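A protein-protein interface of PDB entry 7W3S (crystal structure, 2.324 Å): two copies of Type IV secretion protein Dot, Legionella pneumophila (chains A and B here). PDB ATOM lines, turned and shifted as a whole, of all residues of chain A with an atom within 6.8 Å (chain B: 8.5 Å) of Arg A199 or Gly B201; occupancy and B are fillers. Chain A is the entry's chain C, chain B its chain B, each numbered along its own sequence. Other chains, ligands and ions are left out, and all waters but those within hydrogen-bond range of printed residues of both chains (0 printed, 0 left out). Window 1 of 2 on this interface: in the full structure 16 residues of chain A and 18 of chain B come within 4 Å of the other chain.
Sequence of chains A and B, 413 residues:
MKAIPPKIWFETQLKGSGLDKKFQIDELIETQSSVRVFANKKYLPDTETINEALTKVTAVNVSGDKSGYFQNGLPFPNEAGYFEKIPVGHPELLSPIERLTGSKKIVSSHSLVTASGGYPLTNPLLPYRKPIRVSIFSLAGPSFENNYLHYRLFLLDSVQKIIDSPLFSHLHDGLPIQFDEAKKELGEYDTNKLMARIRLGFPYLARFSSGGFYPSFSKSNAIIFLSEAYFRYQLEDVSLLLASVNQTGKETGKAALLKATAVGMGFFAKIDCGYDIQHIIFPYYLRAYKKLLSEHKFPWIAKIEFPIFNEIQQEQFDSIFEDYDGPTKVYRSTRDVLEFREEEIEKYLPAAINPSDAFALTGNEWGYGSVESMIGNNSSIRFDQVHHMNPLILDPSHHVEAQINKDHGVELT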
ATOM      1  N   TYR A 189      12.282   1.608 -11.056  1.00  0.00           N
ATOM      2  CA  TYR A 189      12.007   0.190 -11.247  1.00  0.00           C
ATOM      3  C   TYR A 189      12.378  -0.609  -9.997  1.00  0.00           C
ATOM      4  O   TYR A 189      12.983  -0.105  -9.050  1.00  0.00           O
ATOM      5  CB  TYR A 189      12.752  -0.341 -12.476  1.00  0.00           C
ATOM      6  CG  TYR A 189      12.295   0.334 -13.745  1.00  0.00           C
ATOM      7  CD1 TYR A 189      10.998   0.157 -14.214  1.00  0.00           C
ATOM      8  CD2 TYR A 189      13.144   1.182 -14.452  1.00  0.00           C
ATOM      9  CE1 TYR A 189      10.561   0.791 -15.363  1.00  0.00           C
ATOM     10  CE2 TYR A 189      12.714   1.817 -15.610  1.00  0.00           C
ATOM     11  CZ  TYR A 189      11.418   1.621 -16.056  1.00  0.00           C
ATOM     12  OH  TYR A 189      10.973   2.246 -17.196  1.00  0.00           O
ATOM     13  N   ASP A 190      11.994  -1.879  -9.999  1.00  0.00           N
ATOM     14  CA  ASP A 190      12.189  -2.733  -8.843  1.00  0.00           C
ATOM     15  C   ASP A 190      13.227  -3.823  -9.071  1.00  0.00           C
ATOM     16  O   ASP A 190      13.576  -4.529  -8.121  1.00  0.00           O
ATOM     17  CB  ASP A 190      10.848  -3.352  -8.429  1.00  0.00           C
ATOM     18  CG  ASP A 190       9.877  -2.323  -7.867  1.00  0.00           C
ATOM     19  OD1 ASP A 190      10.337  -1.272  -7.372  1.00  0.00           O
ATOM     20  OD2 ASP A 190       8.651  -2.564  -7.917  1.00  0.00           O
ATOM     21  N   THR A 191      13.746  -3.962 -10.293  1.00  0.00           N
ATOM     22  CA  THR A 191      14.587  -5.092 -10.656  1.00  0.00           C
ATOM     23  C   THR A 191      15.601  -4.669 -11.707  1.00  0.00           C
ATOM     24  O   THR A 191      15.254  -3.986 -12.671  1.00  0.00           O
ATOM     25  CB  THR A 191      13.744  -6.247 -11.210  1.00  0.00           C
ATOM     26  OG1 THR A 191      12.692  -6.566 -10.289  1.00  0.00           O
ATOM     27  CG2 THR A 191      14.611  -7.484 -11.457  1.00  0.00           C
ATOM     28  N   ALA A 196      16.870  -7.074  -6.828  1.00  0.00           N
ATOM     29  CA  ALA A 196      15.442  -6.846  -6.945  1.00  0.00           C
ATOM     30  C   ALA A 196      14.871  -6.595  -5.562  1.00  0.00           C
ATOM     31  O   ALA A 196      15.280  -7.237  -4.587  1.00  0.00           O
ATOM     32  CB  ALA A 196      14.742  -8.042  -7.602  1.00  0.00           C
ATOM     33  N   ARG A 197      13.961  -5.632  -5.473  1.00  0.00           N
ATOM     34  CA  ARG A 197      13.151  -5.532  -4.273  1.00  0.00           C
ATOM     35  C   ARG A 197      12.272  -6.772  -4.174  1.00  0.00           C
ATOM     36  O   ARG A 197      12.092  -7.515  -5.144  1.00  0.00           O
ATOM     37  CB  ARG A 197      12.301  -4.255  -4.283  1.00  0.00           C
ATOM     38  CG  ARG A 197      12.959  -3.055  -3.587  1.00  0.00           C
ATOM     39  CD  ARG A 197      12.144  -1.749  -3.696  1.00  0.00           C
ATOM     40  NE  ARG A 197      12.373  -1.095  -4.980  1.00  0.00           N
ATOM     41  CZ  ARG A 197      13.314  -0.186  -5.205  1.00  0.00           C
ATOM     42  NH1 ARG A 197      13.447   0.332  -6.412  1.00  0.00           N
ATOM     43  NH2 ARG A 197      14.131   0.196  -4.235  1.00  0.00           N
ATOM     44  N   ILE A 198      11.739  -7.010  -2.986  1.00  0.00           N
ATOM     45  CA  ILE A 198      10.952  -8.206  -2.731  1.00  0.00           C
ATOM     46  C   ILE A 198       9.474  -7.837  -2.825  1.00  0.00           C
ATOM     47  O   ILE A 198       8.933  -7.131  -1.967  1.00  0.00           O
ATOM     48  CB  ILE A 198      11.315  -8.834  -1.383  1.00  0.00           C
ATOM     49  CG1 ILE A 198      12.513  -9.765  -1.585  1.00  0.00           C
ATOM     50  CG2 ILE A 198      10.132  -9.587  -0.792  1.00  0.00           C
ATOM     51  CD1 ILE A 198      13.227 -10.088  -0.331  1.00  0.00           C
ATOM     52  N   ARG A 199       8.834  -8.288  -3.896  1.00  0.00           N
ATOM     53  CA  ARG A 199       7.402  -8.113  -4.069  1.00  0.00           C
ATOM     54  C   ARG A 199       6.681  -9.172  -3.254  1.00  0.00           C
ATOM     55  O   ARG A 199       6.935 -10.369  -3.425  1.00  0.00           O
ATOM     56  CB  ARG A 199       7.019  -8.236  -5.543  1.00  0.00           C
ATOM     57  CG  ARG A 199       8.060  -7.704  -6.504  1.00  0.00           C
ATOM     58  CD  ARG A 199       7.743  -8.065  -7.957  1.00  0.00           C
ATOM     59  NE  ARG A 199       8.730  -7.479  -8.864  1.00  0.00           N
ATOM     60  CZ  ARG A 199       8.434  -6.801  -9.969  1.00  0.00           C
ATOM     61  NH1 ARG A 199       9.409  -6.297 -10.723  1.00  0.00           N
ATOM     62  NH2 ARG A 199       7.166  -6.637 -10.326  1.00  0.00           N
ATOM     63  N   LEU A 200       5.789  -8.741  -2.370  1.00  0.00           N
ATOM     64  CA  LEU A 200       4.877  -9.661  -1.707  1.00  0.00           C
ATOM     65  C   LEU A 200       3.574  -9.843  -2.487  1.00  0.00           C
ATOM     66  O   LEU A 200       2.579 -10.320  -1.928  1.00  0.00           O
ATOM     67  CB  LEU A 200       4.594  -9.171  -0.285  1.00  0.00           C
ATOM     68  CG  LEU A 200       5.765  -9.330   0.681  1.00  0.00           C
ATOM     69  CD1 LEU A 200       5.478  -8.533   1.926  1.00  0.00           C
ATOM     70  CD2 LEU A 200       5.995 -10.804   1.023  1.00  0.00           C
ATOM     71  N   GLY A 201       3.588  -9.528  -3.781  1.00  0.00           N
ATOM     72  CA  GLY A 201       2.412  -9.111  -4.515  1.00  0.00           C
ATOM     73  C   GLY A 201       2.678  -7.710  -5.043  1.00  0.00           C
ATOM     74  O   GLY A 201       3.718  -7.475  -5.669  1.00  0.00           O
ATOM     75  N   PHE A 202       1.783  -6.760  -4.781  1.00  0.00           N
ATOM     76  CA  PHE A 202       2.091  -5.382  -5.164  1.00  0.00           C
ATOM     77  C   PHE A 202       2.875  -4.631  -4.087  1.00  0.00           C
ATOM     78  O   PHE A 202       3.743  -3.821  -4.437  1.00  0.00           O
ATOM     79  CB  PHE A 202       0.825  -4.593  -5.534  1.00  0.00           C
ATOM     80  CG  PHE A 202       0.675  -4.334  -7.014  1.00  0.00           C
ATOM     81  CD1 PHE A 202      -0.249  -5.056  -7.771  1.00  0.00           C
ATOM     82  CD2 PHE A 202       1.500  -3.413  -7.664  1.00  0.00           C
ATOM     83  CE1 PHE A 202      -0.377  -4.827  -9.138  1.00  0.00           C
ATOM     84  CE2 PHE A 202       1.384  -3.202  -9.035  1.00  0.00           C
ATOM     85  CZ  PHE A 202       0.444  -3.910  -9.773  1.00  0.00           C
ATOM     86  N   PRO A 203       2.612  -4.826  -2.795  1.00  0.00           N
ATOM     87  CA  PRO A 203       3.486  -4.228  -1.782  1.00  0.00           C
ATOM     88  C   PRO A 203       4.825  -4.945  -1.685  1.00  0.00           C
ATOM     89  O   PRO A 203       4.978  -6.108  -2.064  1.00  0.00           O
ATOM     90  CB  PRO A 203       2.690  -4.388  -0.479  1.00  0.00           C
ATOM     91  CG  PRO A 203       1.780  -5.521  -0.736  1.00  0.00           C
ATOM     92  CD  PRO A 203       1.382  -5.348  -2.172  1.00  0.00           C
ATOM     93  N   TYR A 204       5.800  -4.212  -1.154  1.00  0.00           N
ATOM     94  CA  TYR A 204       7.142  -4.706  -0.905  1.00  0.00           C
ATOM     95  C   TYR A 204       7.300  -5.124   0.551  1.00  0.00           C
ATOM     96  O   TYR A 204       6.479  -4.807   1.412  1.00  0.00           O
ATOM     97  CB  TYR A 204       8.184  -3.634  -1.236  1.00  0.00           C
ATOM     98  CG  TYR A 204       7.973  -2.938  -2.551  1.00  0.00           C
ATOM     99  CD1 TYR A 204       8.231  -3.587  -3.748  1.00  0.00           C
ATOM    100  CD2 TYR A 204       7.538  -1.623  -2.598  1.00  0.00           C
ATOM    101  CE1 TYR A 204       8.050  -2.954  -4.966  1.00  0.00           C
ATOM    102  CE2 TYR A 204       7.354  -0.968  -3.817  1.00  0.00           C
ATOM    103  CZ  TYR A 204       7.612  -1.637  -4.997  1.00  0.00           C
ATOM    104  OH  TYR A 204       7.428  -0.998  -6.208  1.00  0.00           O
ATOM    105  N   LEU A 205       8.386  -5.840   0.825  1.00  0.00           N
ATOM    106  CA  LEU A 205       8.800  -6.095   2.198  1.00  0.00           C
ATOM    107  C   LEU A 205       9.710  -4.955   2.638  1.00  0.00           C
ATOM    108  O   LEU A 205      10.677  -4.612   1.945  1.00  0.00           O
ATOM    109  CB  LEU A 205       9.506  -7.446   2.341  1.00  0.00           C
ATOM    110  CG  LEU A 205       9.728  -7.903   3.791  1.00  0.00           C
ATOM    111  CD1 LEU A 205       8.426  -7.919   4.597  1.00  0.00           C
ATOM    112  CD2 LEU A 205      10.403  -9.271   3.834  1.00  0.00           C
ATOM    113  N   ASP A 276       7.047 -14.850   3.938  1.00  0.00           N
ATOM    114  CA  ASP A 276       7.565 -15.904   3.076  1.00  0.00           C
ATOM    115  C   ASP A 276       8.185 -15.307   1.822  1.00  0.00           C
ATOM    116  O   ASP A 276       7.548 -14.519   1.118  1.00  0.00           O
ATOM    117  CB  ASP A 276       6.428 -16.853   2.696  1.00  0.00           C
ATOM    118  CG  ASP A 276       6.907 -18.136   2.035  1.00  0.00           C
ATOM    119  OD1 ASP A 276       8.050 -18.200   1.534  1.00  0.00           O
ATOM    120  OD2 ASP A 276       6.112 -19.097   2.014  1.00  0.00           O
ATOM    121  N   HIS A 279       8.809 -17.655  -3.053  1.00  0.00           N
ATOM    122  CA  HIS A 279       8.468 -17.407  -4.455  1.00  0.00           C
ATOM    123  C   HIS A 279       9.519 -16.573  -5.172  1.00  0.00           C
ATOM    124  O   HIS A 279       9.582 -16.609  -6.404  1.00  0.00           O
ATOM    125  CB  HIS A 279       7.113 -16.725  -4.574  1.00  0.00           C
ATOM    126  CG  HIS A 279       7.040 -15.395  -3.894  1.00  0.00           C
ATOM    127  ND1 HIS A 279       6.932 -15.264  -2.524  1.00  0.00           N
ATOM    128  CD2 HIS A 279       7.033 -14.134  -4.396  1.00  0.00           C
ATOM    129  CE1 HIS A 279       6.868 -13.981  -2.212  1.00  0.00           C
ATOM    130  NE2 HIS A 279       6.924 -13.275  -3.329  1.00  0.00           N
ATOM    131  N   ILE A 280      10.356 -15.852  -4.428  1.00  0.00           N
ATOM    132  CA  ILE A 280      11.447 -15.094  -5.030  1.00  0.00           C
ATOM    133  C   ILE A 280      12.757 -15.896  -5.095  1.00  0.00           C
ATOM    134  O   ILE A 280      13.514 -15.763  -6.064  1.00  0.00           O
ATOM    135  CB  ILE A 280      11.608 -13.757  -4.271  1.00  0.00           C
ATOM    136  CG1 ILE A 280      10.570 -12.743  -4.781  1.00  0.00           C
ATOM    137  CG2 ILE A 280      13.007 -13.170  -4.440  1.00  0.00           C
ATOM    138  CD1 ILE A 280       9.987 -11.883  -3.702  1.00  0.00           C
ATOM    139  N   ASP B 190      13.521 -10.039 -17.312  1.00  0.00           N
ATOM    140  CA  ASP B 190      12.208  -9.548 -17.699  1.00  0.00           C
ATOM    141  C   ASP B 190      12.260  -8.256 -18.496  1.00  0.00           C
ATOM    142  O   ASP B 190      11.283  -7.932 -19.175  1.00  0.00           O
ATOM    143  CB  ASP B 190      11.351  -9.294 -16.458  1.00  0.00           C
ATOM    144  CG  ASP B 190      10.804 -10.559 -15.845  1.00  0.00           C
ATOM    145  OD1 ASP B 190      10.932 -11.640 -16.461  1.00  0.00           O
ATOM    146  OD2 ASP B 190      10.226 -10.455 -14.739  1.00  0.00           O
ATOM    147  N   THR B 191      13.364  -7.511 -18.419  1.00  0.00           N
ATOM    148  CA  THR B 191      13.387  -6.108 -18.818  1.00  0.00           C
ATOM    149  C   THR B 191      14.628  -5.822 -19.648  1.00  0.00           C
ATOM    150  O   THR B 191      15.751  -6.009 -19.181  1.00  0.00           O
ATOM    151  CB  THR B 191      13.345  -5.185 -17.585  1.00  0.00           C
ATOM    152  OG1 THR B 191      12.033  -5.202 -17.006  1.00  0.00           O
ATOM    153  CG2 THR B 191      13.714  -3.750 -17.948  1.00  0.00           C
ATOM    154  N   ARG B 197       8.622  -7.563 -20.070  1.00  0.00           N
ATOM    155  CA  ARG B 197       7.466  -8.373 -19.724  1.00  0.00           C
ATOM    156  C   ARG B 197       6.602  -7.604 -18.731  1.00  0.00           C
ATOM    157  O   ARG B 197       7.101  -6.856 -17.890  1.00  0.00           O
ATOM    158  CB  ARG B 197       7.893  -9.717 -19.116  1.00  0.00           C
ATOM    159  CG  ARG B 197       8.800 -10.568 -19.984  1.00  0.00           C
ATOM    160  CD  ARG B 197       8.858 -12.027 -19.502  1.00  0.00           C
ATOM    161  NE  ARG B 197       9.284 -12.927 -20.577  1.00  0.00           N
ATOM    162  CZ  ARG B 197      10.538 -13.325 -20.762  1.00  0.00           C
ATOM    163  NH1 ARG B 197      11.492 -12.921 -19.928  1.00  0.00           N
ATOM    164  NH2 ARG B 197      10.832 -14.131 -21.773  1.00  0.00           N
ATOM    165  N   ILE B 198       5.300  -7.780 -18.830  1.00  0.00           N
ATOM    166  CA  ILE B 198       4.376  -7.066 -17.965  1.00  0.00           C
ATOM    167  C   ILE B 198       4.106  -7.919 -16.734  1.00  0.00           C
ATOM    168  O   ILE B 198       3.806  -9.115 -16.842  1.00  0.00           O
ATOM    169  CB  ILE B 198       3.077  -6.727 -18.714  1.00  0.00           C
ATOM    170  CG1 ILE B 198       3.307  -5.523 -19.635  1.00  0.00           C
ATOM    171  CG2 ILE B 198       1.957  -6.429 -17.747  1.00  0.00           C
ATOM    172  CD1 ILE B 198       2.142  -5.224 -20.538  1.00  0.00           C
ATOM    173  N   ARG B 199       4.230  -7.308 -15.561  1.00  0.00           N
ATOM    174  CA  ARG B 199       3.941  -7.952 -14.291  1.00  0.00           C
ATOM    175  C   ARG B 199       2.892  -7.137 -13.549  1.00  0.00           C
ATOM    176  O   ARG B 199       3.020  -5.918 -13.422  1.00  0.00           O
ATOM    177  CB  ARG B 199       5.219  -8.121 -13.447  1.00  0.00           C
ATOM    178  CG  ARG B 199       6.167  -9.179 -14.036  1.00  0.00           C
ATOM    179  CD  ARG B 199       7.402  -9.429 -13.193  1.00  0.00           C
ATOM    180  NE  ARG B 199       7.089 -10.041 -11.901  1.00  0.00           N
ATOM    181  CZ  ARG B 199       7.998 -10.325 -10.969  1.00  0.00           C
ATOM    182  NH1 ARG B 199       7.629 -10.861  -9.816  1.00  0.00           N
ATOM    183  NH2 ARG B 199       9.279 -10.062 -11.187  1.00  0.00           N
ATOM    184  N   LEU B 200       1.845  -7.807 -13.092  1.00  0.00           N
ATOM    185  CA  LEU B 200       0.774  -7.184 -12.321  1.00  0.00           C
ATOM    186  C   LEU B 200       1.067  -7.289 -10.824  1.00  0.00           C
ATOM    187  O   LEU B 200       0.322  -7.883 -10.051  1.00  0.00           O
ATOM    188  CB  LEU B 200      -0.559  -7.839 -12.662  1.00  0.00           C
ATOM    189  CG  LEU B 200      -1.283  -7.283 -13.889  1.00  0.00           C
ATOM    190  CD1 LEU B 200      -0.321  -6.873 -14.985  1.00  0.00           C
ATOM    191  CD2 LEU B 200      -2.268  -8.296 -14.394  1.00  0.00           C
ATOM    192  N   GLY B 201       2.182  -6.696 -10.406  1.00  0.00           N
ATOM    193  CA  GLY B 201       2.691  -6.918  -9.059  1.00  0.00           C
ATOM    194  C   GLY B 201       3.683  -8.068  -9.020  1.00  0.00           C
ATOM    195  O   GLY B 201       4.847  -7.893  -9.387  1.00  0.00           O
ATOM    196  N   PHE B 202       3.245  -9.255  -8.587  1.00  0.00           N
ATOM    197  CA  PHE B 202       4.120 -10.425  -8.681  1.00  0.00           C
ATOM    198  C   PHE B 202       3.895 -11.238  -9.965  1.00  0.00           C
ATOM    199  O   PHE B 202       4.861 -11.489 -10.698  1.00  0.00           O
ATOM    200  CB  PHE B 202       3.969 -11.327  -7.453  1.00  0.00           C
ATOM    201  CG  PHE B 202       4.668 -12.640  -7.600  1.00  0.00           C
ATOM    202  CD1 PHE B 202       6.048 -12.691  -7.654  1.00  0.00           C
ATOM    203  CD2 PHE B 202       3.947 -13.819  -7.731  1.00  0.00           C
ATOM    204  CE1 PHE B 202       6.694 -13.899  -7.813  1.00  0.00           C
ATOM    205  CE2 PHE B 202       4.590 -15.018  -7.894  1.00  0.00           C
ATOM    206  CZ  PHE B 202       5.960 -15.062  -7.932  1.00  0.00           C
ATOM    207  N   PRO B 203       2.676 -11.673 -10.287  1.00  0.00           N
ATOM    208  CA  PRO B 203       2.503 -12.528 -11.462  1.00  0.00           C
ATOM    209  C   PRO B 203       2.744 -11.772 -12.764  1.00  0.00           C
ATOM    210  O   PRO B 203       2.852 -10.539 -12.809  1.00  0.00           O
ATOM    211  CB  PRO B 203       1.051 -12.998 -11.353  1.00  0.00           C
ATOM    212  CG  PRO B 203       0.386 -12.006 -10.584  1.00  0.00           C
ATOM    213  CD  PRO B 203       1.380 -11.403  -9.638  1.00  0.00           C
ATOM    214  N   TYR B 204       2.837 -12.559 -13.841  1.00  0.00           N
ATOM    215  CA  TYR B 204       2.939 -12.053 -15.202  1.00  0.00           C
ATOM    216  C   TYR B 204       1.551 -11.923 -15.792  1.00  0.00           C
ATOM    217  O   TYR B 204       0.634 -12.656 -15.419  1.00  0.00           O
ATOM    218  CB  TYR B 204       3.768 -12.978 -16.103  1.00  0.00           C
ATOM    219  CG  TYR B 204       5.233 -13.067 -15.744  1.00  0.00           C
ATOM    220  CD1 TYR B 204       6.114 -12.076 -16.132  1.00  0.00           C
ATOM    221  CD2 TYR B 204       5.742 -14.160 -15.030  1.00  0.00           C
ATOM    222  CE1 TYR B 204       7.457 -12.142 -15.806  1.00  0.00           C
ATOM    223  CE2 TYR B 204       7.100 -14.237 -14.694  1.00  0.00           C
ATOM    224  CZ  TYR B 204       7.943 -13.217 -15.090  1.00  0.00           C
ATOM    225  OH  TYR B 204       9.281 -13.245 -14.796  1.00  0.00           O
ATOM    226  N   LEU B 205       1.398 -10.972 -16.711  1.00  0.00           N
ATOM    227  CA  LEU B 205       0.215 -10.916 -17.555  1.00  0.00           C
ATOM    228  C   LEU B 205       0.517 -11.711 -18.819  1.00  0.00           C
ATOM    229  O   LEU B 205       1.509 -11.447 -19.513  1.00  0.00           O
ATOM    230  CB  LEU B 205      -0.182  -9.476 -17.888  1.00  0.00           C
ATOM    231  CG  LEU B 205      -1.377  -9.418 -18.848  1.00  0.00           C
ATOM    232  CD1 LEU B 205      -2.606 -10.059 -18.225  1.00  0.00           C
ATOM    233  CD2 LEU B 205      -1.672  -7.992 -19.285  1.00  0.00           C
ATOM    234  N   ASP B 276      -4.512  -3.771 -15.201  1.00  0.00           N
ATOM    235  CA  ASP B 276      -3.966  -2.429 -15.080  1.00  0.00           C
ATOM    236  C   ASP B 276      -2.463  -2.444 -15.334  1.00  0.00           C
ATOM    237  O   ASP B 276      -1.718  -3.120 -14.623  1.00  0.00           O
ATOM    238  CB  ASP B 276      -4.282  -1.889 -13.691  1.00  0.00           C
ATOM    239  CG  ASP B 276      -4.247  -0.374 -13.625  1.00  0.00           C
ATOM    240  OD1 ASP B 276      -3.673   0.268 -14.535  1.00  0.00           O
ATOM    241  OD2 ASP B 276      -4.800   0.179 -12.653  1.00  0.00           O
ATOM    242  N   HIS B 279       1.076   1.271 -13.973  1.00  0.00           N
ATOM    243  CA  HIS B 279       2.371   1.360 -13.303  1.00  0.00           C
ATOM    244  C   HIS B 279       3.545   1.104 -14.246  1.00  0.00           C
ATOM    245  O   HIS B 279       4.680   1.431 -13.895  1.00  0.00           O
ATOM    246  CB  HIS B 279       2.410   0.385 -12.121  1.00  0.00           C
ATOM    247  CG  HIS B 279       2.257  -1.052 -12.516  1.00  0.00           C
ATOM    248  ND1 HIS B 279       1.096  -1.554 -13.071  1.00  0.00           N
ATOM    249  CD2 HIS B 279       3.126  -2.091 -12.453  1.00  0.00           C
ATOM    250  CE1 HIS B 279       1.258  -2.842 -13.325  1.00  0.00           C
ATOM    251  NE2 HIS B 279       2.476  -3.195 -12.952  1.00  0.00           N
ATOM    252  N   ILE B 280       3.306   0.518 -15.418  1.00  0.00           N
ATOM    253  CA  ILE B 280       4.356   0.319 -16.419  1.00  0.00           C
ATOM    254  C   ILE B 280       4.524   1.536 -17.340  1.00  0.00           C
ATOM    255  O   ILE B 280       5.649   1.913 -17.680  1.00  0.00           O
ATOM    256  CB  ILE B 280       4.038  -0.957 -17.223  1.00  0.00           C
ATOM    257  CG1 ILE B 280       4.390  -2.203 -16.403  1.00  0.00           C
ATOM    258  CG2 ILE B 280       4.770  -0.978 -18.554  1.00  0.00           C
ATOM    259  CD1 ILE B 280       3.394  -3.320 -16.588  1.00  0.00           C
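The guanidinium group of Arg A199 is in hydrogen-bond range of the backbone carbonyl oxygen of Gly B201 (2.8 Å). The backbone NH (N) of Phe B202 sits at hydrogen-bond distance from the backbone carbonyl oxygen (O) of Gly A201 (3.5 Å).
The side-chain carboxylate of Asp B190 is in salt-bridge range of the guanidinium group of Arg B199. The backbone carbonyl oxygen (O) of Phe B202 lies within hydrogen-bond range of the guanidinium group (NE) of Arg B199. A ring nitrogen (NE2) of His B279 lies within hydrogen-bond range of the backbone carbonyl oxygen of Arg B199. The guanidinium group of Arg A199 sits at hydrogen-bond distance from the side-chain hydroxyl of Thr A191, 3.3 Å away. The backbone carbonyl oxygen of Arg A199 sits at hydrogen-bond distance from a ring nitrogen (NE2) of His A279 (2.9 Å).
Among the printed residues, pairs that only touch across the chains: Arg A199 with Arg B199 (3.4 Å), Gly A201 with Gly B201 (3.4 Å), Phe A202 with Leu B200 (3.3 Å), Phe A202 with Gly B201 (3.3 Å), Phe A202 with His B279 (3.8 Å) and His A279 with Phe B202 (3.4 Å).
Of chain B, only Arg B199 and Gly B201 come within 4 Å of Arg A199. Of the printed residues of chain B, Phe A202 touches Leu B200, Gly B201 and His B279. Of the printed residues of chain B, His A279 touches Phe B202. Asp B190 touches none of the printed residues of chain A. Of chain A, only Arg A199 (2.8 Å), Gly A201 (3.4 Å) and Phe A202 (3.3 Å) come within 4 Å of Gly B201. Printed residues of chain A within 4 Å of Phe B202: Gly A201 (3.5 Å) and His A279 (3.4 Å). The nearest residue of chain A that does not touch Gly B201 is Pro A203 (6.6 Å). The nearest printed residue of chain A that does not touch Phe B202 is Arg A199 (4.4 Å).
Of the 16 printed residues of chain A, 4 touch a printed residue of chain B. Printed residues of chain A that touch a printed residue of chain B: Arg A199, Gly A201, Phe A202 and His A279. Hydrophobic or aromatic side chains of chain A that line the printed part of chain B: Phe A202 and His A279.
Arg A199 touches its own counterpart, Arg B199. Arg A199 touches Gly B201, but with the chains exchanged Gly A201 does not touch Arg B199 (6.6 Å). Gly B201 touches its own counterpart, Gly A201. Phe A202 touches His B279, and with the chains exchanged His A279 touches Phe B202. Of the 8 pairs that touch across the chains among the printed residues, 6 have their exchanged pair printed and touching as well.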
